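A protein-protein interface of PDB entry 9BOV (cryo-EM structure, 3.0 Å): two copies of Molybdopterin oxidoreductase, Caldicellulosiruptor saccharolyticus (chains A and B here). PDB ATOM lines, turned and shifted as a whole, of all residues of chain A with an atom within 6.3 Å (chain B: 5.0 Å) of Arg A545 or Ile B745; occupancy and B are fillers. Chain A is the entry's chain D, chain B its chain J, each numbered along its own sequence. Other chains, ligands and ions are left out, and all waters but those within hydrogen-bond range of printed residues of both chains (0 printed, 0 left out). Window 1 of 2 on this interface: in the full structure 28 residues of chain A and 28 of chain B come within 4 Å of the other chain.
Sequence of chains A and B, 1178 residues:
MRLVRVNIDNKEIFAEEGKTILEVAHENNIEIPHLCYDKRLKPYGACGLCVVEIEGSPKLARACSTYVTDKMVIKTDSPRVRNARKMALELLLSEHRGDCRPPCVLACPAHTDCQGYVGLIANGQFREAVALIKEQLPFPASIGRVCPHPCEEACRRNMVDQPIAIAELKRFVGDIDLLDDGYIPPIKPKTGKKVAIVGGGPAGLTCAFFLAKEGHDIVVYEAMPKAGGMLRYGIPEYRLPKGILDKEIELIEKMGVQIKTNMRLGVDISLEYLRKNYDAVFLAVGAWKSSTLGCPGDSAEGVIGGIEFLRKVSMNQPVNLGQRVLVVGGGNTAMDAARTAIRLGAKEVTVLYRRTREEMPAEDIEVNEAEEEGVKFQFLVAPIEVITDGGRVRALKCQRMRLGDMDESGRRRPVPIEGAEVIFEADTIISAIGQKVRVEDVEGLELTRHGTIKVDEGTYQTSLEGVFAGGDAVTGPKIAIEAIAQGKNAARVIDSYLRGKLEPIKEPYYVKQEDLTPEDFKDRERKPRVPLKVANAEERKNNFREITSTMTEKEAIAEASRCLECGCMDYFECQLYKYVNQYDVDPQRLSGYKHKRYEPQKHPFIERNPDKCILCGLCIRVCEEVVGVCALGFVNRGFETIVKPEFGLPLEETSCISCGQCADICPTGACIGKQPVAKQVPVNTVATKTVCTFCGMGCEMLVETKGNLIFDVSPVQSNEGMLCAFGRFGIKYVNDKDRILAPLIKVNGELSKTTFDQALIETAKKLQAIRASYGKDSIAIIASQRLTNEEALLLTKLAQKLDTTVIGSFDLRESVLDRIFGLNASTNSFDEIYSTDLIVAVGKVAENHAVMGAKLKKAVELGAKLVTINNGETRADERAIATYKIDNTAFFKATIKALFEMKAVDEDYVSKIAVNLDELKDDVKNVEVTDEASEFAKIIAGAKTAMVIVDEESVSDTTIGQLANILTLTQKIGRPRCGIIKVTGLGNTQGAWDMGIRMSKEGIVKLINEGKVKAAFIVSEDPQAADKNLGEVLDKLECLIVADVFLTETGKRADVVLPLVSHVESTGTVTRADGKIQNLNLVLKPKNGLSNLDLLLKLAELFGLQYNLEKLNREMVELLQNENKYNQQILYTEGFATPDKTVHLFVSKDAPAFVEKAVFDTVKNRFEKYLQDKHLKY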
ATOM      1  N   GLU A 237      -3.590  -8.306   0.026  1.00  0.00           N
ATOM      2  CA  GLU A 237      -4.556  -9.282  -0.463  1.00  0.00           C
ATOM      3  C   GLU A 237      -5.297  -8.784  -1.698  1.00  0.00           C
ATOM      4  O   GLU A 237      -5.676  -9.590  -2.554  1.00  0.00           O
ATOM      5  CB  GLU A 237      -5.542  -9.632   0.651  1.00  0.00           C
ATOM      6  CG  GLU A 237      -6.658 -10.575   0.238  1.00  0.00           C
ATOM      7  CD  GLU A 237      -6.548 -11.933   0.901  1.00  0.00           C
ATOM      8  OE1 GLU A 237      -5.862 -12.034   1.939  1.00  0.00           O
ATOM      9  OE2 GLU A 237      -7.150 -12.899   0.385  1.00  0.00           O
ATOM     10  N   TYR A 238      -5.511  -7.472  -1.817  1.00  0.00           N
ATOM     11  CA  TYR A 238      -6.220  -6.958  -2.984  1.00  0.00           C
ATOM     12  C   TYR A 238      -5.388  -7.031  -4.256  1.00  0.00           C
ATOM     13  O   TYR A 238      -5.944  -6.864  -5.346  1.00  0.00           O
ATOM     14  CB  TYR A 238      -6.673  -5.515  -2.750  1.00  0.00           C
ATOM     15  CG  TYR A 238      -5.593  -4.578  -2.269  1.00  0.00           C
ATOM     16  CD1 TYR A 238      -4.722  -3.974  -3.163  1.00  0.00           C
ATOM     17  CD2 TYR A 238      -5.461  -4.277  -0.923  1.00  0.00           C
ATOM     18  CE1 TYR A 238      -3.739  -3.115  -2.728  1.00  0.00           C
ATOM     19  CE2 TYR A 238      -4.486  -3.412  -0.480  1.00  0.00           C
ATOM     20  CZ  TYR A 238      -3.624  -2.839  -1.385  1.00  0.00           C
ATOM     21  OH  TYR A 238      -2.646  -1.983  -0.947  1.00  0.00           O
ATOM     22  N   ARG A 239      -4.086  -7.273  -4.147  1.00  0.00           N
ATOM     23  CA  ARG A 239      -3.225  -7.447  -5.308  1.00  0.00           C
ATOM     24  C   ARG A 239      -2.842  -8.901  -5.540  1.00  0.00           C
ATOM     25  O   ARG A 239      -2.726  -9.329  -6.691  1.00  0.00           O
ATOM     26  CB  ARG A 239      -1.961  -6.597  -5.157  1.00  0.00           C
ATOM     27  CG  ARG A 239      -2.114  -5.195  -5.716  1.00  0.00           C
ATOM     28  CD  ARG A 239      -1.065  -4.239  -5.169  1.00  0.00           C
ATOM     29  NE  ARG A 239       0.246  -4.856  -5.008  1.00  0.00           N
ATOM     30  CZ  ARG A 239       1.043  -5.202  -6.009  1.00  0.00           C
ATOM     31  NH1 ARG A 239       0.682  -5.036  -7.271  1.00  0.00           N
ATOM     32  NH2 ARG A 239       2.234  -5.723  -5.737  1.00  0.00           N
ATOM     33  N   ARG A 343      -7.381   1.716   3.067  1.00  0.00           N
ATOM     34  CA  ARG A 343      -8.400   0.698   3.285  1.00  0.00           C
ATOM     35  C   ARG A 343      -8.597   0.359   4.755  1.00  0.00           C
ATOM     36  O   ARG A 343      -9.609  -0.259   5.101  1.00  0.00           O
ATOM     37  CB  ARG A 343      -8.051  -0.571   2.511  1.00  0.00           C
ATOM     38  CG  ARG A 343      -7.996  -0.366   1.016  1.00  0.00           C
ATOM     39  CD  ARG A 343      -7.477  -1.597   0.314  1.00  0.00           C
ATOM     40  NE  ARG A 343      -7.937  -1.665  -1.066  1.00  0.00           N
ATOM     41  CZ  ARG A 343      -7.467  -0.905  -2.044  1.00  0.00           C
ATOM     42  NH1 ARG A 343      -6.523  -0.006  -1.826  1.00  0.00           N
ATOM     43  NH2 ARG A 343      -7.952  -1.055  -3.272  1.00  0.00           N
ATOM     44  N   GLU A 539     -15.677   1.899  -4.561  1.00  0.00           N
ATOM     45  CA  GLU A 539     -16.040   0.632  -3.938  1.00  0.00           C
ATOM     46  C   GLU A 539     -14.819  -0.156  -3.477  1.00  0.00           C
ATOM     47  O   GLU A 539     -14.929  -0.963  -2.547  1.00  0.00           O
ATOM     48  CB  GLU A 539     -16.883  -0.210  -4.899  1.00  0.00           C
ATOM     49  CG  GLU A 539     -16.084  -0.977  -5.942  1.00  0.00           C
ATOM     50  CD  GLU A 539     -16.959  -1.548  -7.041  1.00  0.00           C
ATOM     51  OE1 GLU A 539     -18.195  -1.573  -6.867  1.00  0.00           O
ATOM     52  OE2 GLU A 539     -16.412  -1.971  -8.082  1.00  0.00           O
ATOM     53  N   ARG A 540     -13.660   0.056  -4.100  1.00  0.00           N
ATOM     54  CA  ARG A 540     -12.469  -0.711  -3.760  1.00  0.00           C
ATOM     55  C   ARG A 540     -11.616  -0.058  -2.683  1.00  0.00           C
ATOM     56  O   ARG A 540     -10.773  -0.739  -2.090  1.00  0.00           O
ATOM     57  CB  ARG A 540     -11.613  -0.950  -5.009  1.00  0.00           C
ATOM     58  CG  ARG A 540     -10.539   0.094  -5.236  1.00  0.00           C
ATOM     59  CD  ARG A 540      -9.847  -0.104  -6.568  1.00  0.00           C
ATOM     60  NE  ARG A 540      -8.946   0.999  -6.880  1.00  0.00           N
ATOM     61  CZ  ARG A 540      -8.929   1.648  -8.035  1.00  0.00           C
ATOM     62  NH1 ARG A 540      -9.753   1.328  -9.019  1.00  0.00           N
ATOM     63  NH2 ARG A 540      -8.064   2.642  -8.208  1.00  0.00           N
ATOM     64  N   ASN A 543     -12.350  -2.001   0.948  1.00  0.00           N
ATOM     65  CA  ASN A 543     -12.226  -3.427   1.200  1.00  0.00           C
ATOM     66  C   ASN A 543     -10.903  -3.923   0.640  1.00  0.00           C
ATOM     67  O   ASN A 543     -10.213  -3.220  -0.102  1.00  0.00           O
ATOM     68  CB  ASN A 543     -13.392  -4.204   0.581  1.00  0.00           C
ATOM     69  CG  ASN A 543     -13.654  -3.812  -0.857  1.00  0.00           C
ATOM     70  OD1 ASN A 543     -13.066  -2.862  -1.368  1.00  0.00           O
ATOM     71  ND2 ASN A 543     -14.540  -4.541  -1.518  1.00  0.00           N
ATOM     72  N   PHE A 544     -10.551  -5.154   1.007  1.00  0.00           N
ATOM     73  CA  PHE A 544      -9.345  -5.806   0.519  1.00  0.00           C
ATOM     74  C   PHE A 544      -9.647  -6.837  -0.562  1.00  0.00           C
ATOM     75  O   PHE A 544      -8.894  -7.802  -0.728  1.00  0.00           O
ATOM     76  CB  PHE A 544      -8.587  -6.453   1.676  1.00  0.00           C
ATOM     77  CG  PHE A 544      -7.939  -5.466   2.606  1.00  0.00           C
ATOM     78  CD1 PHE A 544      -8.693  -4.763   3.528  1.00  0.00           C
ATOM     79  CD2 PHE A 544      -6.575  -5.249   2.564  1.00  0.00           C
ATOM     80  CE1 PHE A 544      -8.100  -3.859   4.383  1.00  0.00           C
ATOM     81  CE2 PHE A 544      -5.978  -4.346   3.420  1.00  0.00           C
ATOM     82  CZ  PHE A 544      -6.741  -3.651   4.328  1.00  0.00           C
ATOM     83  N   ARG A 545     -10.742  -6.656  -1.293  1.00  0.00           N
ATOM     84  CA  ARG A 545     -11.055  -7.539  -2.406  1.00  0.00           C
ATOM     85  C   ARG A 545     -10.142  -7.237  -3.587  1.00  0.00           C
ATOM     86  O   ARG A 545      -9.671  -6.111  -3.764  1.00  0.00           O
ATOM     87  CB  ARG A 545     -12.516  -7.385  -2.820  1.00  0.00           C
ATOM     88  CG  ARG A 545     -13.512  -7.690  -1.716  1.00  0.00           C
ATOM     89  CD  ARG A 545     -14.903  -7.935  -2.274  1.00  0.00           C
ATOM     90  NE  ARG A 545     -15.944  -7.569  -1.322  1.00  0.00           N
ATOM     91  CZ  ARG A 545     -16.884  -6.662  -1.550  1.00  0.00           C
ATOM     92  NH1 ARG A 545     -16.947  -6.006  -2.696  1.00  0.00           N
ATOM     93  NH2 ARG A 545     -17.781  -6.406  -0.604  1.00  0.00           N
ATOM     94  N   GLU A 546      -9.894  -8.261  -4.401  1.00  0.00           N
ATOM     95  CA  GLU A 546      -8.983  -8.111  -5.527  1.00  0.00           C
ATOM     96  C   GLU A 546      -9.514  -7.084  -6.517  1.00  0.00           C
ATOM     97  O   GLU A 546     -10.719  -6.999  -6.766  1.00  0.00           O
ATOM     98  CB  GLU A 546      -8.770  -9.453  -6.223  1.00  0.00           C
ATOM     99  CG  GLU A 546      -7.316  -9.750  -6.527  1.00  0.00           C
ATOM    100  CD  GLU A 546      -7.142 -10.762  -7.638  1.00  0.00           C
ATOM    101  OE1 GLU A 546      -8.088 -11.536  -7.892  1.00  0.00           O
ATOM    102  OE2 GLU A 546      -6.060 -10.782  -8.258  1.00  0.00           O
ATOM    103  N   ILE A 547      -8.600  -6.299  -7.082  1.00  0.00           N
ATOM    104  CA  ILE A 547      -8.992  -5.196  -7.952  1.00  0.00           C
ATOM    105  C   ILE A 547      -9.255  -5.687  -9.368  1.00  0.00           C
ATOM    106  O   ILE A 547     -10.330  -5.453  -9.933  1.00  0.00           O
ATOM    107  CB  ILE A 547      -7.912  -4.100  -7.927  1.00  0.00           C
ATOM    108  CG1 ILE A 547      -7.497  -3.804  -6.487  1.00  0.00           C
ATOM    109  CG2 ILE A 547      -8.418  -2.847  -8.610  1.00  0.00           C
ATOM    110  CD1 ILE A 547      -6.706  -2.537  -6.328  1.00  0.00           C
ATOM    111  N   PRO B 743     -22.829 -17.368   2.896  1.00  0.00           N
ATOM    112  CA  PRO B 743     -22.625 -16.017   3.421  1.00  0.00           C
ATOM    113  C   PRO B 743     -23.034 -14.952   2.417  1.00  0.00           C
ATOM    114  O   PRO B 743     -23.118 -15.187   1.210  1.00  0.00           O
ATOM    115  CB  PRO B 743     -21.118 -15.962   3.698  1.00  0.00           C
ATOM    116  CG  PRO B 743     -20.651 -17.373   3.657  1.00  0.00           C
ATOM    117  CD  PRO B 743     -21.556 -18.079   2.709  1.00  0.00           C
ATOM    118  N   LEU B 744     -23.287 -13.759   2.945  1.00  0.00           N
ATOM    119  CA  LEU B 744     -23.664 -12.603   2.146  1.00  0.00           C
ATOM    120  C   LEU B 744     -22.702 -11.463   2.439  1.00  0.00           C
ATOM    121  O   LEU B 744     -22.406 -11.181   3.603  1.00  0.00           O
ATOM    122  CB  LEU B 744     -25.100 -12.168   2.444  1.00  0.00           C
ATOM    123  CG  LEU B 744     -26.213 -13.169   2.138  1.00  0.00           C
ATOM    124  CD1 LEU B 744     -26.551 -13.994   3.363  1.00  0.00           C
ATOM    125  CD2 LEU B 744     -27.444 -12.454   1.625  1.00  0.00           C
ATOM    126  N   ILE B 745     -22.215 -10.813   1.382  1.00  0.00           N
ATOM    127  CA  ILE B 745     -21.358  -9.644   1.514  1.00  0.00           C
ATOM    128  C   ILE B 745     -21.937  -8.526   0.660  1.00  0.00           C
ATOM    129  O   ILE B 745     -22.692  -8.760  -0.284  1.00  0.00           O
ATOM    130  CB  ILE B 745     -19.893  -9.924   1.117  1.00  0.00           C
ATOM    131  CG1 ILE B 745     -19.811 -10.480  -0.303  1.00  0.00           C
ATOM    132  CG2 ILE B 745     -19.244 -10.880   2.105  1.00  0.00           C
ATOM    133  CD1 ILE B 745     -18.398 -10.666  -0.797  1.00  0.00           C
ATOM    134  N   LYS B 746     -21.572  -7.296   1.009  1.00  0.00           N
ATOM    135  CA  LYS B 746     -22.155  -6.105   0.402  1.00  0.00           C
ATOM    136  C   LYS B 746     -21.397  -5.761  -0.874  1.00  0.00           C
ATOM    137  O   LYS B 746     -20.272  -5.254  -0.820  1.00  0.00           O
ATOM    138  CB  LYS B 746     -22.124  -4.939   1.385  1.00  0.00           C
ATOM    139  CG  LYS B 746     -23.398  -4.124   1.424  1.00  0.00           C
ATOM    140  CD  LYS B 746     -23.528  -3.397   2.746  1.00  0.00           C
ATOM    141  CE  LYS B 746     -24.939  -2.886   2.959  1.00  0.00           C
ATOM    142  NZ  LYS B 746     -24.947  -1.587   3.685  1.00  0.00           N
ATOM    143  N   VAL B 747     -22.012  -6.034  -2.021  1.00  0.00           N
ATOM    144  CA  VAL B 747     -21.497  -5.628  -3.321  1.00  0.00           C
ATOM    145  C   VAL B 747     -22.459  -4.606  -3.907  1.00  0.00           C
ATOM    146  O   VAL B 747     -23.672  -4.845  -3.954  1.00  0.00           O
ATOM    147  CB  VAL B 747     -21.322  -6.826  -4.271  1.00  0.00           C
ATOM    148  CG1 VAL B 747     -20.338  -6.483  -5.372  1.00  0.00           C
ATOM    149  CG2 VAL B 747     -20.842  -8.042  -3.499  1.00  0.00           C
ATOM    150  N   GLU B 750     -25.610  -3.867  -1.984  1.00  0.00           N
ATOM    151  CA  GLU B 750     -26.614  -4.898  -1.770  1.00  0.00           C
ATOM    152  C   GLU B 750     -25.938  -6.188  -1.330  1.00  0.00           C
ATOM    153  O   GLU B 750     -24.846  -6.514  -1.800  1.00  0.00           O
ATOM    154  CB  GLU B 750     -27.440  -5.146  -3.037  1.00  0.00           C
ATOM    155  CG  GLU B 750     -28.773  -4.419  -3.062  1.00  0.00           C
ATOM    156  CD  GLU B 750     -29.803  -5.055  -2.148  1.00  0.00           C
ATOM    157  OE1 GLU B 750     -30.248  -6.184  -2.445  1.00  0.00           O
ATOM    158  OE2 GLU B 750     -30.168  -4.426  -1.133  1.00  0.00           O
ATOM    159  N   LEU B 751     -26.584  -6.912  -0.422  1.00  0.00           N
ATOM    160  CA  LEU B 751     -26.039  -8.183   0.035  1.00  0.00           C
ATOM    161  C   LEU B 751     -26.199  -9.242  -1.048  1.00  0.00           C
ATOM    162  O   LEU B 751     -27.290  -9.425  -1.596  1.00  0.00           O
ATOM    163  CB  LEU B 751     -26.734  -8.633   1.318  1.00  0.00           C
ATOM    164  CG  LEU B 751     -26.361  -7.912   2.614  1.00  0.00           C
ATOM    165  CD1 LEU B 751     -27.415  -8.158   3.675  1.00  0.00           C
ATOM    166  CD2 LEU B 751     -25.001  -8.359   3.106  1.00  0.00           C
ATOM    167  N   SER B 752     -25.109  -9.942  -1.354  1.00  0.00           N
ATOM    168  CA  SER B 752     -25.130 -11.016  -2.333  1.00  0.00           C
ATOM    169  C   SER B 752     -24.274 -12.169  -1.835  1.00  0.00           C
ATOM    170  O   SER B 752     -23.354 -11.979  -1.034  1.00  0.00           O
ATOM    171  CB  SER B 752     -24.633 -10.547  -3.704  1.00  0.00           C
ATOM    172  OG  SER B 752     -23.562  -9.633  -3.569  1.00  0.00           O
ATOM    173  N   THR B 754     -21.653 -15.254  -1.431  1.00  0.00           N
ATOM    174  CA  THR B 754     -20.225 -15.391  -1.677  1.00  0.00           C
ATOM    175  C   THR B 754     -19.763 -16.718  -1.085  1.00  0.00           C
ATOM    176  O   THR B 754     -20.575 -17.545  -0.662  1.00  0.00           O
ATOM    177  CB  THR B 754     -19.450 -14.207  -1.088  1.00  0.00           C
ATOM    178  OG1 THR B 754     -18.047 -14.400  -1.305  1.00  0.00           O
ATOM    179  CG2 THR B 754     -19.709 -14.099   0.401  1.00  0.00           C
ATOM    180  N   GLN B 758     -13.963 -15.893   1.400  1.00  0.00           N
ATOM    181  CA  GLN B 758     -14.011 -14.461   1.122  1.00  0.00           C
ATOM    182  C   GLN B 758     -14.776 -13.711   2.204  1.00  0.00           C
ATOM    183  O   GLN B 758     -14.365 -12.625   2.624  1.00  0.00           O
ATOM    184  CB  GLN B 758     -14.638 -14.213  -0.249  1.00  0.00           C
ATOM    185  CG  GLN B 758     -14.632 -12.754  -0.678  1.00  0.00           C
ATOM    186  CD  GLN B 758     -13.239 -12.154  -0.703  1.00  0.00           C
ATOM    187  OE1 GLN B 758     -13.027 -11.030  -0.250  1.00  0.00           O
ATOM    188  NE2 GLN B 758     -12.282 -12.903  -1.239  1.00  0.00           N
ATOM    189  N   ALA B 759     -15.891 -14.277   2.668  1.00  0.00           N
ATOM    190  CA  ALA B 759     -16.678 -13.616   3.703  1.00  0.00           C
ATOM    191  C   ALA B 759     -15.907 -13.507   5.010  1.00  0.00           C
ATOM    192  O   ALA B 759     -15.941 -12.463   5.671  1.00  0.00           O
ATOM    193  CB  ALA B 759     -17.990 -14.363   3.918  1.00  0.00           C
ATOM    194  N   GLU B 762     -13.250 -10.891   4.663  1.00  0.00           N
ATOM    195  CA  GLU B 762     -13.849  -9.565   4.762  1.00  0.00           C
ATOM    196  C   GLU B 762     -14.178  -9.217   6.206  1.00  0.00           C
ATOM    197  O   GLU B 762     -13.954  -8.083   6.645  1.00  0.00           O
ATOM    198  CB  GLU B 762     -15.102  -9.495   3.892  1.00  0.00           C
ATOM    199  CG  GLU B 762     -15.849  -8.180   3.983  1.00  0.00           C
ATOM    200  CD  GLU B 762     -16.229  -7.634   2.623  1.00  0.00           C
ATOM    201  OE1 GLU B 762     -15.641  -8.084   1.616  1.00  0.00           O
ATOM    202  OE2 GLU B 762     -17.112  -6.754   2.559  1.00  0.00           O
ATOM    203  N   ASP B1055     -23.000  -5.614   7.075  1.00  0.00           N
ATOM    204  CA  ASP B1055     -22.060  -5.653   5.963  1.00  0.00           C
ATOM    205  C   ASP B1055     -21.699  -7.078   5.574  1.00  0.00           C
ATOM    206  O   ASP B1055     -21.575  -7.383   4.383  1.00  0.00           O
ATOM    207  CB  ASP B1055     -20.791  -4.875   6.314  1.00  0.00           C
ATOM    208  CG  ASP B1055     -21.082  -3.470   6.787  1.00  0.00           C
ATOM    209  OD1 ASP B1055     -22.246  -3.190   7.140  1.00  0.00           O
ATOM    210  OD2 ASP B1055     -20.148  -2.642   6.804  1.00  0.00           O
ATOM    211  N   VAL B1056     -21.516  -7.955   6.557  1.00  0.00           N
ATOM    212  CA  VAL B1056     -21.254  -9.369   6.327  1.00  0.00           C
ATOM    213  C   VAL B1056     -22.268 -10.169   7.128  1.00  0.00           C
ATOM    214  O   VAL B1056     -22.459  -9.914   8.322  1.00  0.00           O
ATOM    215  CB  VAL B1056     -19.820  -9.768   6.726  1.00  0.00           C
ATOM    216  CG1 VAL B1056     -19.467 -11.121   6.140  1.00  0.00           C
ATOM    217  CG2 VAL B1056     -18.826  -8.719   6.273  1.00  0.00           C
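Of the 14 printed residues of chain B, 4 touch a printed residue of chain A. Hydrophobic or aromatic side chains of chain B within 4 Å of the printed part of chain A: Ile B745. Among the printed residues, 4 pairs touch across the chains.
No position is printed for both chains.
Ile A547 touches none of the printed residues of chain B. Printed residues of chain A within 4 Å of Ile B745: Arg A545. Of the printed residues of chain A, Lys B746 touches Arg A545. Printed residues of chain A within 4 Å of Gln B758: Arg A545. Of the printed residues of chain A, Glu B762 touches Arg A545 (3.0 Å). The nearest printed residue of chain B that does not touch Arg A545 is Val B747 (4.3 Å).
The backbone carbonyl oxygen (O) of Lys B746 is in hydrogen-bond range of the guanidinium group (NH2) of Arg A545, 2.8 Å away. NE of Arg A545 is in salt-bridge range of OE1 of Glu B762 (3.0 Å).
Arg A545 touches Ile B745. OE1 of Gln B758 touches CG of Arg A545 (3.7 Å).
The side-chain amide nitrogen (ND2) of Asn A543 lies close to the guanidinium group (NH1) of Arg A545. The backbone NH (N) of Ser B752 is in hydrogen-bond range of the backbone carbonyl oxygen (O) of Ile B745. The backbone carbonyl oxygen (O) of Asp B1055 is in hydrogen-bond range of the backbone NH (N) of Lys B746 (3.4 Å).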
